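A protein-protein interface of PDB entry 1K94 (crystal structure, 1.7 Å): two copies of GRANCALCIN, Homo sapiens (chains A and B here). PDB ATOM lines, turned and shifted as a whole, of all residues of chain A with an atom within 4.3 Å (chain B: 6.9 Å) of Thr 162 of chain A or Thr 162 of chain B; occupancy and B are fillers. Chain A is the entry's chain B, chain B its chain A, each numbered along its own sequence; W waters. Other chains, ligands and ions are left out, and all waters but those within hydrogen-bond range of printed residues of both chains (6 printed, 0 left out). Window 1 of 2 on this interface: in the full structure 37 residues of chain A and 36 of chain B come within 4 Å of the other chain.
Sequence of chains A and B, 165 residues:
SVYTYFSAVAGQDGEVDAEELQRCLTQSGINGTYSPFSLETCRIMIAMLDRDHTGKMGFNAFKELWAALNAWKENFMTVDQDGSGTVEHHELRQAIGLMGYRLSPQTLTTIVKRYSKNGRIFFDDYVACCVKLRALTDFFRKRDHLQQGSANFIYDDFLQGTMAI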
ATOM      1  N   LYS A 132     -18.421  10.071  13.985  1.00  0.00           N
ATOM      2  CA  LYS A 132     -18.867  10.967  12.923  1.00  0.00           C
ATOM      3  C   LYS A 132     -19.528  10.226  11.762  1.00  0.00           C
ATOM      4  O   LYS A 132     -20.533  10.688  11.218  1.00  0.00           O
ATOM      5  CB  LYS A 132     -17.692  11.815  12.425  1.00  0.00           C
ATOM      6  CG  LYS A 132     -18.090  12.919  11.455  1.00  0.00           C
ATOM      7  CD  LYS A 132     -16.965  13.933  11.300  1.00  0.00           C
ATOM      8  CE  LYS A 132     -17.342  15.041  10.327  1.00  0.00           C
ATOM      9  NZ  LYS A 132     -16.245  16.049  10.215  1.00  0.00           N
ATOM     10  N   LEU A 136     -23.347  11.162  10.860  1.00  0.00           N
ATOM     11  CA  LEU A 136     -23.664  11.742   9.560  1.00  0.00           C
ATOM     12  C   LEU A 136     -24.457  10.793   8.672  1.00  0.00           C
ATOM     13  O   LEU A 136     -25.288  11.234   7.872  1.00  0.00           O
ATOM     14  CB  LEU A 136     -22.383  12.195   8.847  1.00  0.00           C
ATOM     15  CG  LEU A 136     -21.661  13.389   9.488  1.00  0.00           C
ATOM     16  CD1 LEU A 136     -20.437  13.751   8.654  1.00  0.00           C
ATOM     17  CD2 LEU A 136     -22.607  14.585   9.585  1.00  0.00           C
ATOM     18  N   PHE A 158     -29.083  21.073   6.350  1.00  0.00           N
ATOM     19  CA  PHE A 158     -27.756  20.534   6.085  1.00  0.00           C
ATOM     20  C   PHE A 158     -26.775  21.063   7.133  1.00  0.00           C
ATOM     21  O   PHE A 158     -26.009  20.300   7.724  1.00  0.00           O
ATOM     22  CB  PHE A 158     -27.298  20.961   4.684  1.00  0.00           C
ATOM     23  CG  PHE A 158     -25.873  20.588   4.359  1.00  0.00           C
ATOM     24  CD1 PHE A 158     -25.547  19.299   3.946  1.00  0.00           C
ATOM     25  CD2 PHE A 158     -24.861  21.539   4.450  1.00  0.00           C
ATOM     26  CE1 PHE A 158     -24.232  18.964   3.625  1.00  0.00           C
ATOM     27  CE2 PHE A 158     -23.541  21.215   4.131  1.00  0.00           C
ATOM     28  CZ  PHE A 158     -23.228  19.926   3.718  1.00  0.00           C
ATOM     29  N   LEU A 159     -26.800  22.369   7.369  1.00  0.00           N
ATOM     30  CA  LEU A 159     -25.894  22.957   8.350  1.00  0.00           C
ATOM     31  C   LEU A 159     -26.143  22.476   9.775  1.00  0.00           C
ATOM     32  O   LEU A 159     -25.198  22.209  10.515  1.00  0.00           O
ATOM     33  CB  LEU A 159     -25.964  24.487   8.306  1.00  0.00           C
ATOM     34  CG  LEU A 159     -25.187  25.163   7.174  1.00  0.00           C
ATOM     35  CD1 LEU A 159     -25.310  26.678   7.313  1.00  0.00           C
ATOM     36  CD2 LEU A 159     -23.718  24.749   7.233  1.00  0.00           C
ATOM     37  N   GLN A 160     -27.404  22.358  10.174  1.00  0.00           N
ATOM     38  CA  GLN A 160     -27.666  21.903  11.531  1.00  0.00           C
ATOM     39  C   GLN A 160     -27.135  20.493  11.757  1.00  0.00           C
ATOM     40  O   GLN A 160     -26.483  20.224  12.768  1.00  0.00           O
ATOM     41  CB  GLN A 160     -29.159  21.940  11.856  1.00  0.00           C
ATOM     42  CG  GLN A 160     -29.475  21.229  13.164  1.00  0.00           C
ATOM     43  CD  GLN A 160     -30.899  21.421  13.620  1.00  0.00           C
ATOM     44  OE1 GLN A 160     -31.836  21.351  12.824  1.00  0.00           O
ATOM     45  NE2 GLN A 160     -31.074  21.645  14.917  1.00  0.00           N
ATOM     46  N   GLY A 161     -27.412  19.598  10.815  1.00  0.00           N
ATOM     47  CA  GLY A 161     -26.955  18.226  10.948  1.00  0.00           C
ATOM     48  C   GLY A 161     -25.444  18.075  10.930  1.00  0.00           C
ATOM     49  O   GLY A 161     -24.892  17.239  11.654  1.00  0.00           O
ATOM     50  N   THR A 162     -24.769  18.875  10.107  1.00  0.00           N
ATOM     51  CA  THR A 162     -23.313  18.799   9.998  1.00  0.00           C
ATOM     52  C   THR A 162     -22.559  19.614  11.050  1.00  0.00           C
ATOM     53  O   THR A 162     -21.482  19.210  11.494  1.00  0.00           O
ATOM     54  CB  THR A 162     -22.835  19.208   8.582  1.00  0.00           C
ATOM     55  OG1 THR A 162     -23.334  20.510   8.251  1.00  0.00           O
ATOM     56  CG2 THR A 162     -23.336  18.205   7.547  1.00  0.00           C
ATOM     57  N   MET A 163     -23.112  20.753  11.457  1.00  0.00           N
ATOM     58  CA  MET A 163     -22.454  21.553  12.482  1.00  0.00           C
ATOM     59  C   MET A 163     -22.609  20.864  13.837  1.00  0.00           C
ATOM     60  O   MET A 163     -21.816  21.078  14.752  1.00  0.00           O
ATOM     61  CB  MET A 163     -23.053  22.961  12.553  1.00  0.00           C
ATOM     62  CG  MET A 163     -22.683  23.874  11.389  1.00  0.00           C
ATOM     63  SD  MET A 163     -20.917  24.289  11.282  1.00  0.00           S
ATOM     64  CE  MET A 163     -20.758  25.413  12.661  1.00  0.00           C
ATOM     65  N   ALA A 164     -23.636  20.030  13.962  1.00  0.00           N
ATOM     66  CA  ALA A 164     -23.887  19.320  15.211  1.00  0.00           C
ATOM     67  C   ALA A 164     -22.777  18.344  15.569  1.00  0.00           C
ATOM     68  O   ALA A 164     -22.524  18.091  16.748  1.00  0.00           O
ATOM     69  CB  ALA A 164     -25.208  18.568  15.126  1.00  0.00           C
ATOM     70  N   ILE A 165     -22.107  17.798  14.559  1.00  0.00           N
ATOM     71  CA  ILE A 165     -21.061  16.815  14.815  1.00  0.00           C
ATOM     72  C   ILE A 165     -19.653  17.349  14.556  1.00  0.00           C
ATOM     73  O   ILE A 165     -19.075  17.954  15.484  1.00  0.00           O
ATOM     74  CB  ILE A 165     -21.294  15.555  13.945  1.00  0.00           C
ATOM     75  CG1 ILE A 165     -22.777  15.166  13.975  1.00  0.00           C
ATOM     76  CG2 ILE A 165     -20.445  14.397  14.454  1.00  0.00           C
ATOM     77  CD1 ILE A 165     -23.331  14.887  15.379  1.00  0.00           C
ATOM     78  OXT ILE A 165     -19.154  17.166  13.427  1.00  0.00           O
ATOM     79  N   ARG B 114     -22.881  23.026  20.777  1.00  0.00           N
ATOM     80  CA  ARG B 114     -21.743  22.278  20.262  1.00  0.00           C
ATOM     81  C   ARG B 114     -20.395  22.941  20.516  1.00  0.00           C
ATOM     82  O   ARG B 114     -19.401  22.259  20.759  1.00  0.00           O
ATOM     83  CB  ARG B 114     -21.917  22.052  18.757  1.00  0.00           C
ATOM     84  CG  ARG B 114     -20.745  21.351  18.083  1.00  0.00           C
ATOM     85  CD  ARG B 114     -20.576  19.921  18.578  1.00  0.00           C
ATOM     86  NE  ARG B 114     -19.461  19.258  17.907  1.00  0.00           N
ATOM     87  CZ  ARG B 114     -18.184  19.576  18.090  1.00  0.00           C
ATOM     88  NH1 ARG B 114     -17.856  20.547  18.937  1.00  0.00           N
ATOM     89  NH2 ARG B 114     -17.235  18.936  17.419  1.00  0.00           N
ATOM     90  N   TYR B 115     -20.370  24.271  20.477  1.00  0.00           N
ATOM     91  CA  TYR B 115     -19.131  25.017  20.656  1.00  0.00           C
ATOM     92  C   TYR B 115     -18.889  25.627  22.031  1.00  0.00           C
ATOM     93  O   TYR B 115     -17.849  26.240  22.259  1.00  0.00           O
ATOM     94  CB  TYR B 115     -19.047  26.104  19.581  1.00  0.00           C
ATOM     95  CG  TYR B 115     -18.755  25.542  18.208  1.00  0.00           C
ATOM     96  CD1 TYR B 115     -17.441  25.316  17.796  1.00  0.00           C
ATOM     97  CD2 TYR B 115     -19.790  25.175  17.349  1.00  0.00           C
ATOM     98  CE1 TYR B 115     -17.165  24.734  16.558  1.00  0.00           C
ATOM     99  CE2 TYR B 115     -19.523  24.591  16.110  1.00  0.00           C
ATOM    100  CZ  TYR B 115     -18.210  24.373  15.723  1.00  0.00           C
ATOM    101  OH  TYR B 115     -17.943  23.792  14.505  1.00  0.00           O
ATOM    102  N   LYS B 132     -15.732  26.208  10.003  1.00  0.00           N
ATOM    103  CA  LYS B 132     -16.587  25.107   9.585  1.00  0.00           C
ATOM    104  C   LYS B 132     -17.816  25.592   8.818  1.00  0.00           C
ATOM    105  O   LYS B 132     -18.244  24.950   7.858  1.00  0.00           O
ATOM    106  CB  LYS B 132     -17.006  24.271  10.796  1.00  0.00           C
ATOM    107  CG  LYS B 132     -17.605  22.923  10.423  1.00  0.00           C
ATOM    108  CD  LYS B 132     -17.752  22.035  11.635  1.00  0.00           C
ATOM    109  CE  LYS B 132     -18.278  20.662  11.252  1.00  0.00           C
ATOM    110  NZ  LYS B 132     -18.383  19.771  12.444  1.00  0.00           N
ATOM    111  N   LEU B 136     -18.294  24.113   5.104  1.00  0.00           N
ATOM    112  CA  LEU B 136     -19.501  23.361   4.780  1.00  0.00           C
ATOM    113  C   LEU B 136     -20.332  24.079   3.721  1.00  0.00           C
ATOM    114  O   LEU B 136     -20.934  23.440   2.856  1.00  0.00           O
ATOM    115  CB  LEU B 136     -20.339  23.132   6.046  1.00  0.00           C
ATOM    116  CG  LEU B 136     -19.789  22.061   6.995  1.00  0.00           C
ATOM    117  CD1 LEU B 136     -20.513  22.111   8.339  1.00  0.00           C
ATOM    118  CD2 LEU B 136     -19.946  20.691   6.347  1.00  0.00           C
ATOM    119  N   PHE B 139     -18.822  23.589   0.231  1.00  0.00           N
ATOM    120  CA  PHE B 139     -19.183  22.277  -0.283  1.00  0.00           C
ATOM    121  C   PHE B 139     -20.628  22.270  -0.775  1.00  0.00           C
ATOM    122  O   PHE B 139     -20.921  21.779  -1.862  1.00  0.00           O
ATOM    123  CB  PHE B 139     -18.988  21.218   0.813  1.00  0.00           C
ATOM    124  CG  PHE B 139     -19.500  19.848   0.439  1.00  0.00           C
ATOM    125  CD1 PHE B 139     -19.146  19.263  -0.770  1.00  0.00           C
ATOM    126  CD2 PHE B 139     -20.335  19.147   1.301  1.00  0.00           C
ATOM    127  CE1 PHE B 139     -19.621  17.997  -1.119  1.00  0.00           C
ATOM    128  CE2 PHE B 139     -20.814  17.883   0.963  1.00  0.00           C
ATOM    129  CZ  PHE B 139     -20.458  17.306  -0.247  1.00  0.00           C
ATOM    130  N   PHE B 153     -27.387  15.372  -2.772  1.00  0.00           N
ATOM    131  CA  PHE B 153     -26.076  14.783  -2.532  1.00  0.00           C
ATOM    132  C   PHE B 153     -26.198  13.278  -2.579  1.00  0.00           C
ATOM    133  O   PHE B 153     -27.136  12.712  -2.020  1.00  0.00           O
ATOM    134  CB  PHE B 153     -25.527  15.122  -1.140  1.00  0.00           C
ATOM    135  CG  PHE B 153     -25.283  16.575  -0.902  1.00  0.00           C
ATOM    136  CD1 PHE B 153     -26.319  17.413  -0.515  1.00  0.00           C
ATOM    137  CD2 PHE B 153     -23.997  17.099  -1.013  1.00  0.00           C
ATOM    138  CE1 PHE B 153     -26.078  18.754  -0.236  1.00  0.00           C
ATOM    139  CE2 PHE B 153     -23.748  18.439  -0.738  1.00  0.00           C
ATOM    140  CZ  PHE B 153     -24.791  19.268  -0.348  1.00  0.00           C
ATOM    141  N   TYR B 155     -24.823   9.841  -1.275  1.00  0.00           N
ATOM    142  CA  TYR B 155     -24.180   9.479  -0.011  1.00  0.00           C
ATOM    143  C   TYR B 155     -22.661   9.628   0.019  1.00  0.00           C
ATOM    144  O   TYR B 155     -22.110  10.280   0.908  1.00  0.00           O
ATOM    145  CB  TYR B 155     -24.558   8.042   0.355  1.00  0.00           C
ATOM    146  CG  TYR B 155     -23.943   7.529   1.638  1.00  0.00           C
ATOM    147  CD1 TYR B 155     -23.140   6.391   1.638  1.00  0.00           C
ATOM    148  CD2 TYR B 155     -24.203   8.153   2.863  1.00  0.00           C
ATOM    149  CE1 TYR B 155     -22.614   5.880   2.818  1.00  0.00           C
ATOM    150  CE2 TYR B 155     -23.676   7.649   4.056  1.00  0.00           C
ATOM    151  CZ  TYR B 155     -22.886   6.511   4.022  1.00  0.00           C
ATOM    152  OH  TYR B 155     -22.377   5.994   5.188  1.00  0.00           O
ATOM    153  N   ASP B 157     -20.598  11.317  -1.907  1.00  0.00           N
ATOM    154  CA  ASP B 157     -20.181  12.707  -2.085  1.00  0.00           C
ATOM    155  C   ASP B 157     -20.394  13.432  -0.756  1.00  0.00           C
ATOM    156  O   ASP B 157     -19.541  14.188  -0.292  1.00  0.00           O
ATOM    157  CB  ASP B 157     -21.038  13.357  -3.175  1.00  0.00           C
ATOM    158  CG  ASP B 157     -20.657  14.798  -3.449  1.00  0.00           C
ATOM    159  OD1 ASP B 157     -21.569  15.590  -3.771  1.00  0.00           O
ATOM    160  OD2 ASP B 157     -19.458  15.141  -3.366  1.00  0.00           O
ATOM    161  N   PHE B 158     -21.549  13.183  -0.151  1.00  0.00           N
ATOM    162  CA  PHE B 158     -21.902  13.784   1.127  1.00  0.00           C
ATOM    163  C   PHE B 158     -20.810  13.542   2.168  1.00  0.00           C
ATOM    164  O   PHE B 158     -20.371  14.470   2.850  1.00  0.00           O
ATOM    165  CB  PHE B 158     -23.217  13.187   1.625  1.00  0.00           C
ATOM    166  CG  PHE B 158     -23.655  13.707   2.962  1.00  0.00           C
ATOM    167  CD1 PHE B 158     -24.136  15.004   3.099  1.00  0.00           C
ATOM    168  CD2 PHE B 158     -23.602  12.890   4.087  1.00  0.00           C
ATOM    169  CE1 PHE B 158     -24.564  15.480   4.336  1.00  0.00           C
ATOM    170  CE2 PHE B 158     -24.027  13.356   5.324  1.00  0.00           C
ATOM    171  CZ  PHE B 158     -24.511  14.654   5.449  1.00  0.00           C
ATOM    172  N   LEU B 159     -20.378  12.292   2.287  1.00  0.00           N
ATOM    173  CA  LEU B 159     -19.347  11.941   3.253  1.00  0.00           C
ATOM    174  C   LEU B 159     -17.992  12.523   2.893  1.00  0.00           C
ATOM    175  O   LEU B 159     -17.242  12.935   3.769  1.00  0.00           O
ATOM    176  CB  LEU B 159     -19.228  10.421   3.392  1.00  0.00           C
ATOM    177  CG  LEU B 159     -20.400   9.693   4.051  1.00  0.00           C
ATOM    178  CD1 LEU B 159     -20.049   8.222   4.213  1.00  0.00           C
ATOM    179  CD2 LEU B 159     -20.702  10.314   5.409  1.00  0.00           C
ATOM    180  N   GLN B 160     -17.670  12.552   1.605  1.00  0.00           N
ATOM    181  CA  GLN B 160     -16.391  13.099   1.176  1.00  0.00           C
ATOM    182  C   GLN B 160     -16.235  14.557   1.576  1.00  0.00           C
ATOM    183  O   GLN B 160     -15.189  14.968   2.076  1.00  0.00           O
ATOM    184  CB  GLN B 160     -16.241  12.972  -0.340  1.00  0.00           C
ATOM    185  CG  GLN B 160     -15.481  11.747  -0.770  1.00  0.00           C
ATOM    186  CD  GLN B 160     -15.363  11.643  -2.273  1.00  0.00           C
ATOM    187  OE1 GLN B 160     -14.933  12.586  -2.939  1.00  0.00           O
ATOM    188  NE2 GLN B 160     -15.743  10.492  -2.818  1.00  0.00           N
ATOM    189  N   GLY B 161     -17.283  15.340   1.355  1.00  0.00           N
ATOM    190  CA  GLY B 161     -17.219  16.749   1.685  1.00  0.00           C
ATOM    191  C   GLY B 161     -17.272  17.047   3.168  1.00  0.00           C
ATOM    192  O   GLY B 161     -16.623  17.980   3.636  1.00  0.00           O
ATOM    193  N   THR B 162     -18.029  16.252   3.916  1.00  0.00           N
ATOM    194  CA  THR B 162     -18.170  16.484   5.349  1.00  0.00           C
ATOM    195  C   THR B 162     -17.107  15.819   6.214  1.00  0.00           C
ATOM    196  O   THR B 162     -16.714  16.369   7.240  1.00  0.00           O
ATOM    197  CB  THR B 162     -19.549  16.031   5.838  1.00  0.00           C
ATOM    198  OG1 THR B 162     -19.713  14.631   5.581  1.00  0.00           O
ATOM    199  CG2 THR B 162     -20.635  16.798   5.114  1.00  0.00           C
ATOM    200  N   MET B 163     -16.646  14.640   5.811  1.00  0.00           N
ATOM    201  CA  MET B 163     -15.626  13.941   6.590  1.00  0.00           C
ATOM    202  C   MET B 163     -14.247  14.576   6.413  1.00  0.00           C
ATOM    203  O   MET B 163     -13.342  14.338   7.216  1.00  0.00           O
ATOM    204  CB  MET B 163     -15.559  12.465   6.186  1.00  0.00           C
ATOM    205  CG  MET B 163     -16.818  11.660   6.495  1.00  0.00           C
ATOM    206  SD  MET B 163     -17.183  11.562   8.260  1.00  0.00           S
ATOM    207  CE  MET B 163     -15.823  10.549   8.856  1.00  0.00           C
ATOM    208  N   ALA B 164     -14.086  15.378   5.366  1.00  0.00           N
ATOM    209  CA  ALA B 164     -12.803  16.030   5.102  1.00  0.00           C
ATOM    210  C   ALA B 164     -12.581  17.235   6.005  1.00  0.00           C
ATOM    211  O   ALA B 164     -11.448  17.683   6.194  1.00  0.00           O
ATOM    212  CB  ALA B 164     -12.725  16.463   3.641  1.00  0.00           C
ATOM    213  N   ILE B 165     -13.668  17.759   6.557  1.00  0.00           N
ATOM    214  CA  ILE B 165     -13.603  18.927   7.429  1.00  0.00           C
ATOM    215  C   ILE B 165     -13.401  18.529   8.887  1.00  0.00           C
ATOM    216  O   ILE B 165     -12.422  19.012   9.497  1.00  0.00           O
ATOM    217  CB  ILE B 165     -14.887  19.768   7.297  1.00  0.00           C
ATOM    218  CG1 ILE B 165     -15.070  20.187   5.836  1.00  0.00           C
ATOM    219  CG2 ILE B 165     -14.806  20.999   8.197  1.00  0.00           C
ATOM    220  CD1 ILE B 165     -16.372  20.906   5.556  1.00  0.00           C
ATOM    221  OXT ILE B 165     -14.221  17.745   9.406  1.00  0.00           O
HETATM  222  O   HOH W   1     -16.574  17.401  12.804  1.00  0.00           O
HETATM  223  O   HOH W   2     -17.910  18.317   8.809  1.00  0.00           O
HETATM  224  O   HOH W   3     -13.783  17.010  12.041  1.00  0.00           O
HETATM  225  O   HOH W   4     -19.864  17.171  10.821  1.00  0.00           O
HETATM  226  O   HOH W   5     -13.902  14.396   9.757  1.00  0.00           O
HETATM  227  O   HOH W   6     -19.328  21.473  14.444  1.00  0.00           O
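Lys 132 of chain A touches Met 163 of chain B, and with the chains exchanged Met 163 of chain A touches Lys 132 of chain B. Leu 136 of chain A touches Phe 158 of chain B, and with the chains exchanged Phe 158 of chain A touches Leu 136 of chain B. Leu 136 of chain A touches Thr 162 of chain B, and with the chains exchanged Thr 162 of chain A touches Leu 136 of chain B. Leu 159 of chain A touches Leu 136 of chain B, but with the chains exchanged Leu 136 of chain A does not touch Leu 159 of chain B (4.3 Å). Positions printed for both chains: 132, 136, 158, 159, 160, 161, 162, 163, 164 and 165.
Hydrophobic or aromatic side chains of chain B that line the printed part of chain A: Tyr 115, Leu 136, Phe 139, Phe 158 and Met 163. Of the 10 printed residues of chain A, 8 touch a printed residue of chain B. Printed residues of chain A that touch a printed residue of chain B: Lys 132, Leu 136, Phe 158, Leu 159, Thr 162, Met 163, Ala 164 and Ile 165. Hydrophobic or aromatic side chains of chain A within 4 Å of the printed part of chain B: Leu 136, Phe 158, Leu 159 and Met 163. Among the printed residues, 20 pairs touch across the chains. Among the printed residues, no Asp or Glu carboxylate lies within 4 Å of a Lys or Arg side-chain nitrogen of the other chain.
Leu 136 of chain A touches Thr 162 of chain B (CD1 to OG1, 3.3 Å). O of Leu 136 of chain B touches CE2 of Phe 158 of chain A (3.7 Å). CD2 of Phe 139 of chain B touches CZ of Phe 158 of chain A (3.8 Å). Phe 158 of chain B touches Phe 158 of chain A (CE1 to CE1, 3.6 Å). Leu 159 of chain A touches Leu 136 of chain B. Thr 162 of chain A touches Leu 136 of chain B. CG2 of Thr 162 of chain A touches CG2 of Thr 162 of chain B (3.9 Å). Met 163 of chain A touches Arg 114 of chain B (O to CG, 3.5 Å). Tyr 115 of chain B touches Met 163 of chain A (OH to CE, 3.7 Å). Met 163 of chain A touches Leu 136 of chain B (SD to CD1, 3.7 Å).
The backbone carbonyl oxygen of Ala 164 of chain A lies close to the guanidinium group of Arg 114 of chain B (3.5 Å). The chain-end carboxylate of Ile 165 of chain A lies within salt-bridge range of the guanidinium group of Arg 114 of chain B (2.8 Å). The side-chain amino group (NZ) of Lys 132 of chain B is in hydrogen-bond range of the backbone carbonyl oxygen (O) of Thr 162 of chain A (3.3 Å). NZ of Lys 132 of chain B is in salt-bridge range of OXT of Ile 165 of chain A (2.9 Å). O of Thr 162 of chain B lies within hydrogen-bond range of NZ of Lys 132 of chain A (3.0 Å). OXT of Ile 165 of chain B lies within salt-bridge range of NZ of Lys 132 of chain A (2.8 Å).
The side-chain hydroxyl of Thr 162 of chain B is in hydrogen-bond range of the backbone carbonyl oxygen of Phe 158 of chain B, at 2.8 Å. The side-chain hydroxyl (OG1) of Thr 162 of chain A sits at hydrogen-bond distance from the backbone carbonyl oxygen (O) of Phe 158 of chain A, 2.7 Å away. O of Leu 159 of chain A lies within hydrogen-bond range of OG1 of Thr 162 of chain A (3.4 Å).
Thr 162 of chain A touches three residues of chain B. Of the printed residues of chain A, Thr 162 of chain B touches Lys 132, Leu 136 and Thr 162. Gly 161 of chain A touches none of the printed residues of chain B. Of the printed residues of chain B, Ile 165 of chain A touches Arg 114 (2.8 Å) and Lys 132 (2.9 Å). Of the printed residues of chain A, Met 163 of chain B touches Lys 132 and Leu 136. Of the printed residues of chain A, Tyr 115 of chain B touches Met 163 (3.7 Å). Printed residues of chain B within 4 Å of Met 163 of chain A: Arg 114, Tyr 115, Lys 132 and Leu 136. The nearest residue of chain B that does not touch Thr 162 of chain A is Phe 158 of chain B (4.3 Å). The nearest printed residue of chain A that does not touch Thr 162 of chain B is Phe 158 of chain A (4.3 Å). The nearest printed residue of chain A that does not touch Ile 165 of chain B is Ile 165 of chain A (6.4 Å).
Water W6 lies within hydrogen-bond range of O of Met 163 of chain A (2.5 Å), OH of Tyr 115 of chain B (2.7 Å) and NZ of Lys 132 of chain B (2.8 Å). Water W5 lies within hydrogen-bond range of the backbone carbonyl oxygen of Met 163 of chain B (2.6 Å), the side-chain amino group of Lys 132 of chain A (2.9 Å) and the chain-end carboxylate of Ile 165 of chain B (3.4 Å). Water W1 lies within hydrogen-bond range of OXT of Ile 165 of chain A (2.7 Å), NZ of Lys 132 of chain A (2.9 Å) and NZ of Lys 132 of chain B (3.0 Å). Water W4 lies within hydrogen-bond range of the backbone carbonyl oxygen of Thr 162 of chain A (2.7 Å), the chain-end carboxylate of Ile 165 of chain A (2.7 Å) and the side-chain amino group of Lys 132 of chain B (3.4 Å). Water W3 bridges the chain-end carboxylate (OXT) of Ile 165 of chain B (2.8 Å) and the side-chain amino group (NZ) of Lys 132 of chain A (3.2 Å). Water W2 lies within hydrogen-bond range of O of Thr 162 of chain B (2.8 Å) and NZ of Lys 132 of chain A (3.1 Å).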
